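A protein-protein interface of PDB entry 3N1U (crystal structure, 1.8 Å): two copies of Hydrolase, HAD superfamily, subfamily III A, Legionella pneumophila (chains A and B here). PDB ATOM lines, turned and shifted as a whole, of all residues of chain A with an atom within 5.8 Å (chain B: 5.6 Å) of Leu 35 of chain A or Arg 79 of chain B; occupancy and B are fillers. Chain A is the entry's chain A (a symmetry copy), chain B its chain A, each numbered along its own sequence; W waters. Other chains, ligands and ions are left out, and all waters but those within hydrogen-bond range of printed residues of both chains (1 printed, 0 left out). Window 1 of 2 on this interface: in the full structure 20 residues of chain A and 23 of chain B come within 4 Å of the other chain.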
ATOM      1  N   ASP A  27     -12.544   3.372  17.360  1.00  0.00           N
ATOM      2  CA  ASP A  27     -11.283   3.463  16.647  1.00  0.00           C
ATOM      3  C   ASP A  27     -11.141   4.822  15.987  1.00  0.00           C
ATOM      4  O   ASP A  27     -12.016   5.175  15.191  1.00  0.00           O
ATOM      5  CB  ASP A  27     -11.266   2.404  15.546  1.00  0.00           C
ATOM      6  CG  ASP A  27     -11.209   0.998  16.105  1.00  0.00           C
ATOM      7  OD1 ASP A  27     -10.129   0.584  16.593  1.00  0.00           O
ATOM      8  OD2 ASP A  27     -12.223   0.309  16.059  1.00  0.00           O
ATOM      9  N   ASP A  32      -6.002   6.259  18.716  1.00  0.00           N
ATOM     10  CA  ASP A  32      -5.290   6.957  17.659  1.00  0.00           C
ATOM     11  C   ASP A  32      -5.710   6.532  16.306  1.00  0.00           C
ATOM     12  O   ASP A  32      -5.262   7.114  15.296  1.00  0.00           O
ATOM     13  CB  ASP A  32      -3.716   6.669  17.691  1.00  0.00           C
ATOM     14  CG  ASP A  32      -3.348   5.205  18.134  1.00  0.00           C
ATOM     15  OD1 ASP A  32      -4.154   4.261  17.974  1.00  0.00           O
ATOM     16  OD2 ASP A  32      -2.226   4.992  18.728  1.00  0.00           O
ATOM     17  N   GLY A  33      -6.525   5.488  16.230  1.00  0.00           N
ATOM     18  CA  GLY A  33      -6.847   4.969  14.880  1.00  0.00           C
ATOM     19  C   GLY A  33      -6.063   3.730  14.497  1.00  0.00           C
ATOM     20  O   GLY A  33      -6.340   3.121  13.484  1.00  0.00           O
ATOM     21  N   LEU A  34      -5.026   3.371  15.282  1.00  0.00           N
ATOM     22  CA  LEU A  34      -4.162   2.270  14.856  1.00  0.00           C
ATOM     23  C   LEU A  34      -4.734   0.963  15.317  1.00  0.00           C
ATOM     24  O   LEU A  34      -5.287   0.858  16.412  1.00  0.00           O
ATOM     25  CB  LEU A  34      -2.732   2.457  15.467  1.00  0.00           C
ATOM     26  CG  LEU A  34      -2.000   3.688  14.883  1.00  0.00           C
ATOM     27  CD1 LEU A  34      -0.549   3.742  15.526  1.00  0.00           C
ATOM     28  CD2 LEU A  34      -1.871   3.643  13.262  1.00  0.00           C
ATOM     29  N   LEU A  35      -4.513  -0.046  14.503  1.00  0.00           N
ATOM     30  CA  LEU A  35      -4.809  -1.431  14.804  1.00  0.00           C
ATOM     31  C   LEU A  35      -3.506  -2.157  14.834  1.00  0.00           C
ATOM     32  O   LEU A  35      -2.806  -2.300  13.785  1.00  0.00           O
ATOM     33  CB  LEU A  35      -5.690  -1.992  13.687  1.00  0.00           C
ATOM     34  CG  LEU A  35      -6.914  -1.169  13.306  1.00  0.00           C
ATOM     35  CD1 LEU A  35      -7.509  -1.846  12.006  1.00  0.00           C
ATOM     36  CD2 LEU A  35      -7.957  -1.127  14.464  1.00  0.00           C
ATOM     37  N   HIS A  36      -3.091  -2.607  16.018  1.00  0.00           N
ATOM     38  CA  HIS A  36      -1.804  -3.273  16.110  1.00  0.00           C
ATOM     39  C   HIS A  36      -2.062  -4.774  15.963  1.00  0.00           C
ATOM     40  O   HIS A  36      -2.995  -5.297  16.595  1.00  0.00           O
ATOM     41  CB  HIS A  36      -1.123  -3.002  17.453  1.00  0.00           C
ATOM     42  CG  HIS A  36      -1.209  -1.576  17.910  1.00  0.00           C
ATOM     43  ND1 HIS A  36      -0.469  -0.564  17.334  1.00  0.00           N
ATOM     44  CD2 HIS A  36      -1.898  -1.006  18.935  1.00  0.00           C
ATOM     45  CE1 HIS A  36      -0.720   0.575  17.965  1.00  0.00           C
ATOM     46  NE2 HIS A  36      -1.579   0.341  18.944  1.00  0.00           N
ATOM     47  N   ILE A  37      -1.352  -5.422  15.042  1.00  0.00           N
ATOM     48  CA  ILE A  37      -1.647  -6.803  14.691  1.00  0.00           C
ATOM     49  C   ILE A  37      -0.364  -7.580  14.788  1.00  0.00           C
ATOM     50  O   ILE A  37       0.692  -7.169  14.255  1.00  0.00           O
ATOM     51  CB  ILE A  37      -2.268  -6.910  13.254  1.00  0.00           C
ATOM     52  CG1 ILE A  37      -3.611  -6.139  13.157  1.00  0.00           C
ATOM     53  CG2 ILE A  37      -2.525  -8.393  12.894  1.00  0.00           C
ATOM     54  CD1 ILE A  37      -4.159  -6.142  11.653  1.00  0.00           C
ATOM     55  N   LEU A  44      -4.406  -5.315  19.102  1.00  0.00           N
ATOM     56  CA  LEU A  44      -4.442  -4.445  20.270  1.00  0.00           C
ATOM     57  C   LEU A  44      -4.914  -3.111  19.786  1.00  0.00           C
ATOM     58  O   LEU A  44      -4.857  -2.828  18.575  1.00  0.00           O
ATOM     59  CB  LEU A  44      -3.037  -4.296  20.868  1.00  0.00           C
ATOM     60  CG  LEU A  44      -2.310  -5.535  21.315  1.00  0.00           C
ATOM     61  CD1 LEU A  44      -1.348  -5.999  20.208  1.00  0.00           C
ATOM     62  CD2 LEU A  44      -1.462  -5.179  22.555  1.00  0.00           C
ATOM     63  N   LYS A  45      -5.442  -2.315  20.702  1.00  0.00           N
ATOM     64  CA  LYS A  45      -5.672  -0.891  20.450  1.00  0.00           C
ATOM     65  C   LYS A  45      -5.085  -0.133  21.639  1.00  0.00           C
ATOM     66  O   LYS A  45      -4.916  -0.697  22.732  1.00  0.00           O
ATOM     67  CB  LYS A  45      -7.164  -0.527  20.400  1.00  0.00           C
ATOM     68  CG  LYS A  45      -8.012  -1.420  19.476  1.00  0.00           C
ATOM     69  CD  LYS A  45      -9.491  -1.062  19.554  1.00  0.00           C
ATOM     70  CE  LYS A  45     -10.318  -1.916  18.592  1.00  0.00           C
ATOM     71  NZ  LYS A  45      -9.869  -1.920  17.121  1.00  0.00           N
ATOM     72  N   LYS B  45       2.789  -4.963  13.350  1.00  0.00           N
ATOM     73  CA  LYS B  45       2.761  -3.677  12.650  1.00  0.00           C
ATOM     74  C   LYS B  45       1.452  -2.992  13.038  1.00  0.00           C
ATOM     75  O   LYS B  45       0.488  -3.653  13.457  1.00  0.00           O
ATOM     76  CB  LYS B  45       2.732  -3.831  11.121  1.00  0.00           C
ATOM     77  CG  LYS B  45       3.805  -4.776  10.550  1.00  0.00           C
ATOM     78  CD  LYS B  45       3.652  -4.953   9.045  1.00  0.00           C
ATOM     79  CE  LYS B  45       4.756  -5.848   8.479  1.00  0.00           C
ATOM     80  NZ  LYS B  45       6.202  -5.437   8.801  1.00  0.00           N
ATOM     81  N   SER B  46       1.380  -1.695  12.749  1.00  0.00           N
ATOM     82  CA  SER B  46       0.218  -0.890  13.155  1.00  0.00           C
ATOM     83  C   SER B  46      -0.388  -0.272  11.914  1.00  0.00           C
ATOM     84  O   SER B  46       0.324   0.481  11.198  1.00  0.00           O
ATOM     85  CB  SER B  46       0.713   0.225  14.112  1.00  0.00           C
ATOM     86  OG  SER B  46       1.317  -0.414  15.236  1.00  0.00           O
ATOM     87  N   PHE B  47      -1.680  -0.565  11.640  1.00  0.00           N
ATOM     88  CA  PHE B  47      -2.371  -0.037  10.447  1.00  0.00           C
ATOM     89  C   PHE B  47      -3.418   0.981  10.897  1.00  0.00           C
ATOM     90  O   PHE B  47      -3.794   0.971  12.055  1.00  0.00           O
ATOM     91  CB  PHE B  47      -3.071  -1.195   9.727  1.00  0.00           C
ATOM     92  CG  PHE B  47      -2.119  -2.267   9.258  1.00  0.00           C
ATOM     93  CD1 PHE B  47      -1.441  -2.116   8.034  1.00  0.00           C
ATOM     94  CD2 PHE B  47      -1.897  -3.409  10.026  1.00  0.00           C
ATOM     95  CE1 PHE B  47      -0.491  -3.067   7.572  1.00  0.00           C
ATOM     96  CE2 PHE B  47      -0.968  -4.382   9.595  1.00  0.00           C
ATOM     97  CZ  PHE B  47      -0.275  -4.242   8.346  1.00  0.00           C
ATOM     98  N   HIS B  48      -3.933   1.827  10.005  1.00  0.00           N
ATOM     99  CA  HIS B  48      -4.820   2.872  10.450  1.00  0.00           C
ATOM    100  C   HIS B  48      -6.232   2.596   9.902  1.00  0.00           C
ATOM    101  O   HIS B  48      -6.409   2.280   8.725  1.00  0.00           O
ATOM    102  CB  HIS B  48      -4.305   4.239   9.947  1.00  0.00           C
ATOM    103  CG  HIS B  48      -4.970   5.387  10.645  1.00  0.00           C
ATOM    104  ND1 HIS B  48      -6.296   5.767  10.389  1.00  0.00           N
ATOM    105  CD2 HIS B  48      -4.519   6.204  11.616  1.00  0.00           C
ATOM    106  CE1 HIS B  48      -6.616   6.768  11.196  1.00  0.00           C
ATOM    107  NE2 HIS B  48      -5.557   7.050  11.955  1.00  0.00           N
ATOM    108  N   VAL B  49      -7.220   2.705  10.759  1.00  0.00           N
ATOM    109  CA  VAL B  49      -8.606   2.438  10.337  1.00  0.00           C
ATOM    110  C   VAL B  49      -9.115   3.322   9.215  1.00  0.00           C
ATOM    111  O   VAL B  49      -9.995   2.912   8.465  1.00  0.00           O
ATOM    112  CB  VAL B  49      -9.580   2.551  11.519  1.00  0.00           C
ATOM    113  CG1 VAL B  49      -9.349   1.331  12.452  1.00  0.00           C
ATOM    114  CG2 VAL B  49      -9.501   3.945  12.202  1.00  0.00           C
ATOM    115  N   ASP B  51      -7.437   4.361   6.675  1.00  0.00           N
ATOM    116  CA  ASP B  51      -6.866   3.813   5.443  1.00  0.00           C
ATOM    117  C   ASP B  51      -7.588   2.552   5.078  1.00  0.00           C
ATOM    118  O   ASP B  51      -7.865   2.324   3.902  1.00  0.00           O
ATOM    119  CB  ASP B  51      -5.383   3.459   5.673  1.00  0.00           C
ATOM    120  CG  ASP B  51      -4.485   4.641   5.812  1.00  0.00           C
ATOM    121  OD1 ASP B  51      -4.760   5.745   5.301  1.00  0.00           O
ATOM    122  OD2 ASP B  51      -3.405   4.432   6.459  1.00  0.00           O
ATOM    123  N   GLY B  52      -7.887   1.707   6.064  1.00  0.00           N
ATOM    124  CA  GLY B  52      -8.675   0.487   5.782  1.00  0.00           C
ATOM    125  C   GLY B  52     -10.061   0.835   5.180  1.00  0.00           C
ATOM    126  O   GLY B  52     -10.493   0.228   4.211  1.00  0.00           O
ATOM    127  N   ALA B  74       3.582 -12.939   8.613  1.00  0.00           N
ATOM    128  CA  ALA B  74       2.162 -13.245   8.645  1.00  0.00           C
ATOM    129  C   ALA B  74       1.259 -12.061   9.092  1.00  0.00           C
ATOM    130  O   ALA B  74       0.081 -12.067   8.781  1.00  0.00           O
ATOM    131  CB  ALA B  74       1.898 -14.485   9.500  1.00  0.00           C
ATOM    132  N   VAL B  75       1.812 -11.043   9.773  1.00  0.00           N
ATOM    133  CA  VAL B  75       1.034  -9.801   9.976  1.00  0.00           C
ATOM    134  C   VAL B  75       0.342  -9.319   8.676  1.00  0.00           C
ATOM    135  O   VAL B  75      -0.827  -8.928   8.691  1.00  0.00           O
ATOM    136  CB  VAL B  75       1.933  -8.651  10.508  1.00  0.00           C
ATOM    137  CG1 VAL B  75       1.118  -7.321  10.581  1.00  0.00           C
ATOM    138  CG2 VAL B  75       2.501  -9.006  11.869  1.00  0.00           C
ATOM    139  N   VAL B  76       1.091  -9.313   7.567  1.00  0.00           N
ATOM    140  CA  VAL B  76       0.589  -8.819   6.293  1.00  0.00           C
ATOM    141  C   VAL B  76      -0.631  -9.664   5.860  1.00  0.00           C
ATOM    142  O   VAL B  76      -1.657  -9.115   5.508  1.00  0.00           O
ATOM    143  CB  VAL B  76       1.709  -8.805   5.208  1.00  0.00           C
ATOM    144  CG1 VAL B  76       1.154  -8.465   3.810  1.00  0.00           C
ATOM    145  CG2 VAL B  76       2.858  -7.815   5.655  1.00  0.00           C
ATOM    146  N   ASP B  77      -0.516 -10.997   5.934  1.00  0.00           N
ATOM    147  CA  ASP B  77      -1.600 -11.895   5.526  1.00  0.00           C
ATOM    148  C   ASP B  77      -2.860 -11.649   6.350  1.00  0.00           C
ATOM    149  O   ASP B  77      -3.998 -11.588   5.787  1.00  0.00           O
ATOM    150  CB  ASP B  77      -1.162 -13.360   5.661  1.00  0.00           C
ATOM    151  CG  ASP B  77       0.086 -13.649   4.843  1.00  0.00           C
ATOM    152  OD1 ASP B  77       0.025 -13.617   3.587  1.00  0.00           O
ATOM    153  OD2 ASP B  77       1.115 -13.928   5.460  1.00  0.00           O
ATOM    154  N   HIS B  78      -2.670 -11.473   7.657  1.00  0.00           N
ATOM    155  CA  HIS B  78      -3.825 -11.205   8.540  1.00  0.00           C
ATOM    156  C   HIS B  78      -4.509  -9.919   8.182  1.00  0.00           C
ATOM    157  O   HIS B  78      -5.735  -9.865   8.109  1.00  0.00           O
ATOM    158  CB  HIS B  78      -3.429 -11.181  10.016  1.00  0.00           C
ATOM    159  CG  HIS B  78      -3.076 -12.530  10.550  1.00  0.00           C
ATOM    160  ND1 HIS B  78      -1.813 -12.848  11.014  1.00  0.00           N
ATOM    161  CD2 HIS B  78      -3.826 -13.645  10.698  1.00  0.00           C
ATOM    162  CE1 HIS B  78      -1.805 -14.106  11.426  1.00  0.00           C
ATOM    163  NE2 HIS B  78      -3.010 -14.613  11.239  1.00  0.00           N
ATOM    164  N   ARG B  79      -3.725  -8.885   7.920  1.00  0.00           N
ATOM    165  CA  ARG B  79      -4.326  -7.608   7.500  1.00  0.00           C
ATOM    166  C   ARG B  79      -5.033  -7.676   6.142  1.00  0.00           C
ATOM    167  O   ARG B  79      -6.119  -7.112   5.960  1.00  0.00           O
ATOM    168  CB  ARG B  79      -3.289  -6.477   7.518  1.00  0.00           C
ATOM    169  CG  ARG B  79      -3.881  -5.084   7.173  1.00  0.00           C
ATOM    170  CD  ARG B  79      -4.880  -4.587   8.263  1.00  0.00           C
ATOM    171  NE  ARG B  79      -5.299  -3.191   8.059  1.00  0.00           N
ATOM    172  CZ  ARG B  79      -6.484  -2.716   8.473  1.00  0.00           C
ATOM    173  NH1 ARG B  79      -7.370  -3.529   9.089  1.00  0.00           N
ATOM    174  NH2 ARG B  79      -6.808  -1.461   8.238  1.00  0.00           N
ATOM    175  N   MET B  80      -4.421  -8.353   5.165  1.00  0.00           N
ATOM    176  CA  MET B  80      -5.057  -8.447   3.870  1.00  0.00           C
ATOM    177  C   MET B  80      -6.380  -9.194   3.964  1.00  0.00           C
ATOM    178  O   MET B  80      -7.335  -8.827   3.284  1.00  0.00           O
ATOM    179  CB  MET B  80      -4.153  -9.179   2.875  1.00  0.00           C
ATOM    180  CG  MET B  80      -2.835  -8.533   2.636  1.00  0.00           C
ATOM    181  SD  MET B  80      -2.963  -6.793   1.736  1.00  0.00           S
ATOM    182  CE  MET B  80      -2.965  -5.673   3.394  1.00  0.00           C
ATOM    183  N   GLU B  81      -6.397 -10.271   4.745  1.00  0.00           N
ATOM    184  CA  GLU B  81      -7.634 -11.051   4.981  1.00  0.00           C
ATOM    185  C   GLU B  81      -8.718 -10.183   5.637  1.00  0.00           C
ATOM    186  O   GLU B  81      -9.874 -10.249   5.239  1.00  0.00           O
ATOM    187  CB  GLU B  81      -7.353 -12.277   5.853  1.00  0.00           C
ATOM    188  CG  GLU B  81      -8.656 -13.050   6.189  1.00  0.00           C
ATOM    189  CD  GLU B  81      -8.453 -14.266   7.103  1.00  0.00           C
ATOM    190  OE1 GLU B  81      -9.223 -15.232   6.924  1.00  0.00           O
ATOM    191  OE2 GLU B  81      -7.553 -14.258   7.996  1.00  0.00           O
ATOM    192  N   GLN B  82      -8.329  -9.343   6.611  1.00  0.00           N
ATOM    193  CA  GLN B  82      -9.256  -8.417   7.294  1.00  0.00           C
ATOM    194  C   GLN B  82      -9.906  -7.499   6.299  1.00  0.00           C
ATOM    195  O   GLN B  82     -11.118  -7.254   6.389  1.00  0.00           O
ATOM    196  CB  GLN B  82      -8.551  -7.497   8.332  1.00  0.00           C
ATOM    197  CG  GLN B  82      -8.305  -8.129   9.669  1.00  0.00           C
ATOM    198  CD  GLN B  82      -7.734  -7.152  10.703  1.00  0.00           C
ATOM    199  OE1 GLN B  82      -7.259  -6.044  10.381  1.00  0.00           O
ATOM    200  NE2 GLN B  82      -7.758  -7.583  11.966  1.00  0.00           N
ATOM    201  N   LEU B  83      -9.104  -6.973   5.376  1.00  0.00           N
ATOM    202  CA  LEU B  83      -9.603  -6.014   4.392  1.00  0.00           C
ATOM    203  C   LEU B  83     -10.233  -6.633   3.131  1.00  0.00           C
ATOM    204  O   LEU B  83     -10.807  -5.923   2.309  1.00  0.00           O
ATOM    205  CB  LEU B  83      -8.486  -5.050   4.007  1.00  0.00           C
ATOM    206  CG  LEU B  83      -8.045  -4.110   5.134  1.00  0.00           C
ATOM    207  CD1 LEU B  83      -6.929  -3.195   4.625  1.00  0.00           C
ATOM    208  CD2 LEU B  83      -9.223  -3.322   5.736  1.00  0.00           C
ATOM    209  N   GLY B  84     -10.161  -7.954   3.010  1.00  0.00           N
ATOM    210  CA  GLY B  84     -10.671  -8.661   1.798  1.00  0.00           C
ATOM    211  C   GLY B  84      -9.879  -8.367   0.540  1.00  0.00           C
ATOM    212  O   GLY B  84     -10.397  -8.446  -0.599  1.00  0.00           O
HETATM  213  O   HOH W   1      -3.213   8.482  13.872  1.00  0.00           O
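The backbone NH (N) of Ile 37 of chain A sits at hydrogen-bond distance from the backbone carbonyl oxygen (O) of Lys 45 of chain B. ND1 of His 36 of chain A is in hydrogen-bond range of OG of Ser 46 of chain B (2.8 Å). The backbone NH of Leu 35 of chain A lies within hydrogen-bond range of the backbone carbonyl oxygen of Phe 47 of chain B (2.7 Å). O of Asp 32 of chain A sits at hydrogen-bond distance from NE2 of His 48 of chain B, 3.4 Å away. The backbone carbonyl oxygen (O) of Gly 33 of chain A is in hydrogen-bond range of the backbone NH (N) of Val 49 of chain B (2.9 Å).
1 position is printed for both chains. Of the 19 pairs that touch across the chains among the printed residues, none has its exchanged pair printed and touching as well.
The side-chain amide oxygen (OE1) of Gln 82 of chain B lies within hydrogen-bond range of the guanidinium group (NH1) of Arg 79 of chain B (2.8 Å). The side-chain amino group (NZ) of Lys 45 of chain A is in salt-bridge range of the side-chain carboxylate (OD1) of Asp 27 of chain A (2.6 Å). The side-chain carboxylate (OD1) of Asp 32 of chain A lies within hydrogen-bond range of the backbone NH (N) of Leu 34 of chain A, 3.0 Å away. O of His 36 of chain A sits at hydrogen-bond distance from N of Leu 44 of chain A.
Hydrophobic or aromatic side chains of chain A within 4 Å of the printed part of chain B: Leu 34, Leu 35, His 36 and Ile 37. Among the printed residues, no Asp or Glu carboxylate lies within 4 Å of a Lys or Arg side-chain nitrogen of the other chain.
CG1 of Val 49 of chain B touches CB of Asp 27 of chain A, 3.8 Å away. Phe 47 of chain B touches Gly 33 of chain A. Leu 34 of chain A touches Ser 46 of chain B. O of Phe 47 of chain B touches CA of Leu 34 of chain A, at 3.1 Å. Leu 35 of chain A touches Val 49 of chain B (CD2 to CG1, 3.5 Å). NH1 of Arg 79 of chain B touches CD1 of Leu 35 of chain A, at 3.4 Å. O of Lys 45 of chain B touches CA of His 36 of chain A, at 3.5 Å. CD1 of Ile 37 of chain A touches CD2 of Phe 47 of chain B, at 3.9 Å. CG2 of Val 75 of chain B touches O of Ile 37 of chain A, at 3.5 Å. Arg 79 of chain B touches Ile 37 of chain A.
Of the printed residues of chain B, Asp 27 of chain A touches Val 49. Of the printed residues of chain B, Ile 37 of chain A touches Lys 45 (3.0 Å), Phe 47 (3.9 Å), Val 75 (3.5 Å), Arg 79 (3.8 Å) and Gln 82 (3.4 Å). Of the printed residues of chain A, Lys 45 of chain B touches Leu 35 (3.6 Å), His 36 (3.5 Å) and Ile 37 (3.0 Å). Of the printed residues of chain A, Phe 47 of chain B touches Gly 33, Leu 34, Leu 35 and Ile 37. Arg 79 of chain B touches just these residues of chain A: Leu 35 and Ile 37. Printed residues of chain A within 4 Å of Gln 82 of chain B: Ile 37. The nearest residue of chain B that does not touch Leu 35 of chain A is Gln 82 of chain B (4.5 Å). The nearest printed residue of chain A that does not touch Arg 79 of chain B is Gly 33 of chain A (7.0 Å). The nearest printed residue of chain B that does not touch Leu 34 of chain A is His 48 of chain B (4.03 Å).
Water W1 lies within hydrogen-bond range of O of Asp 32 of chain A and NE2 of His 48 of chain B.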
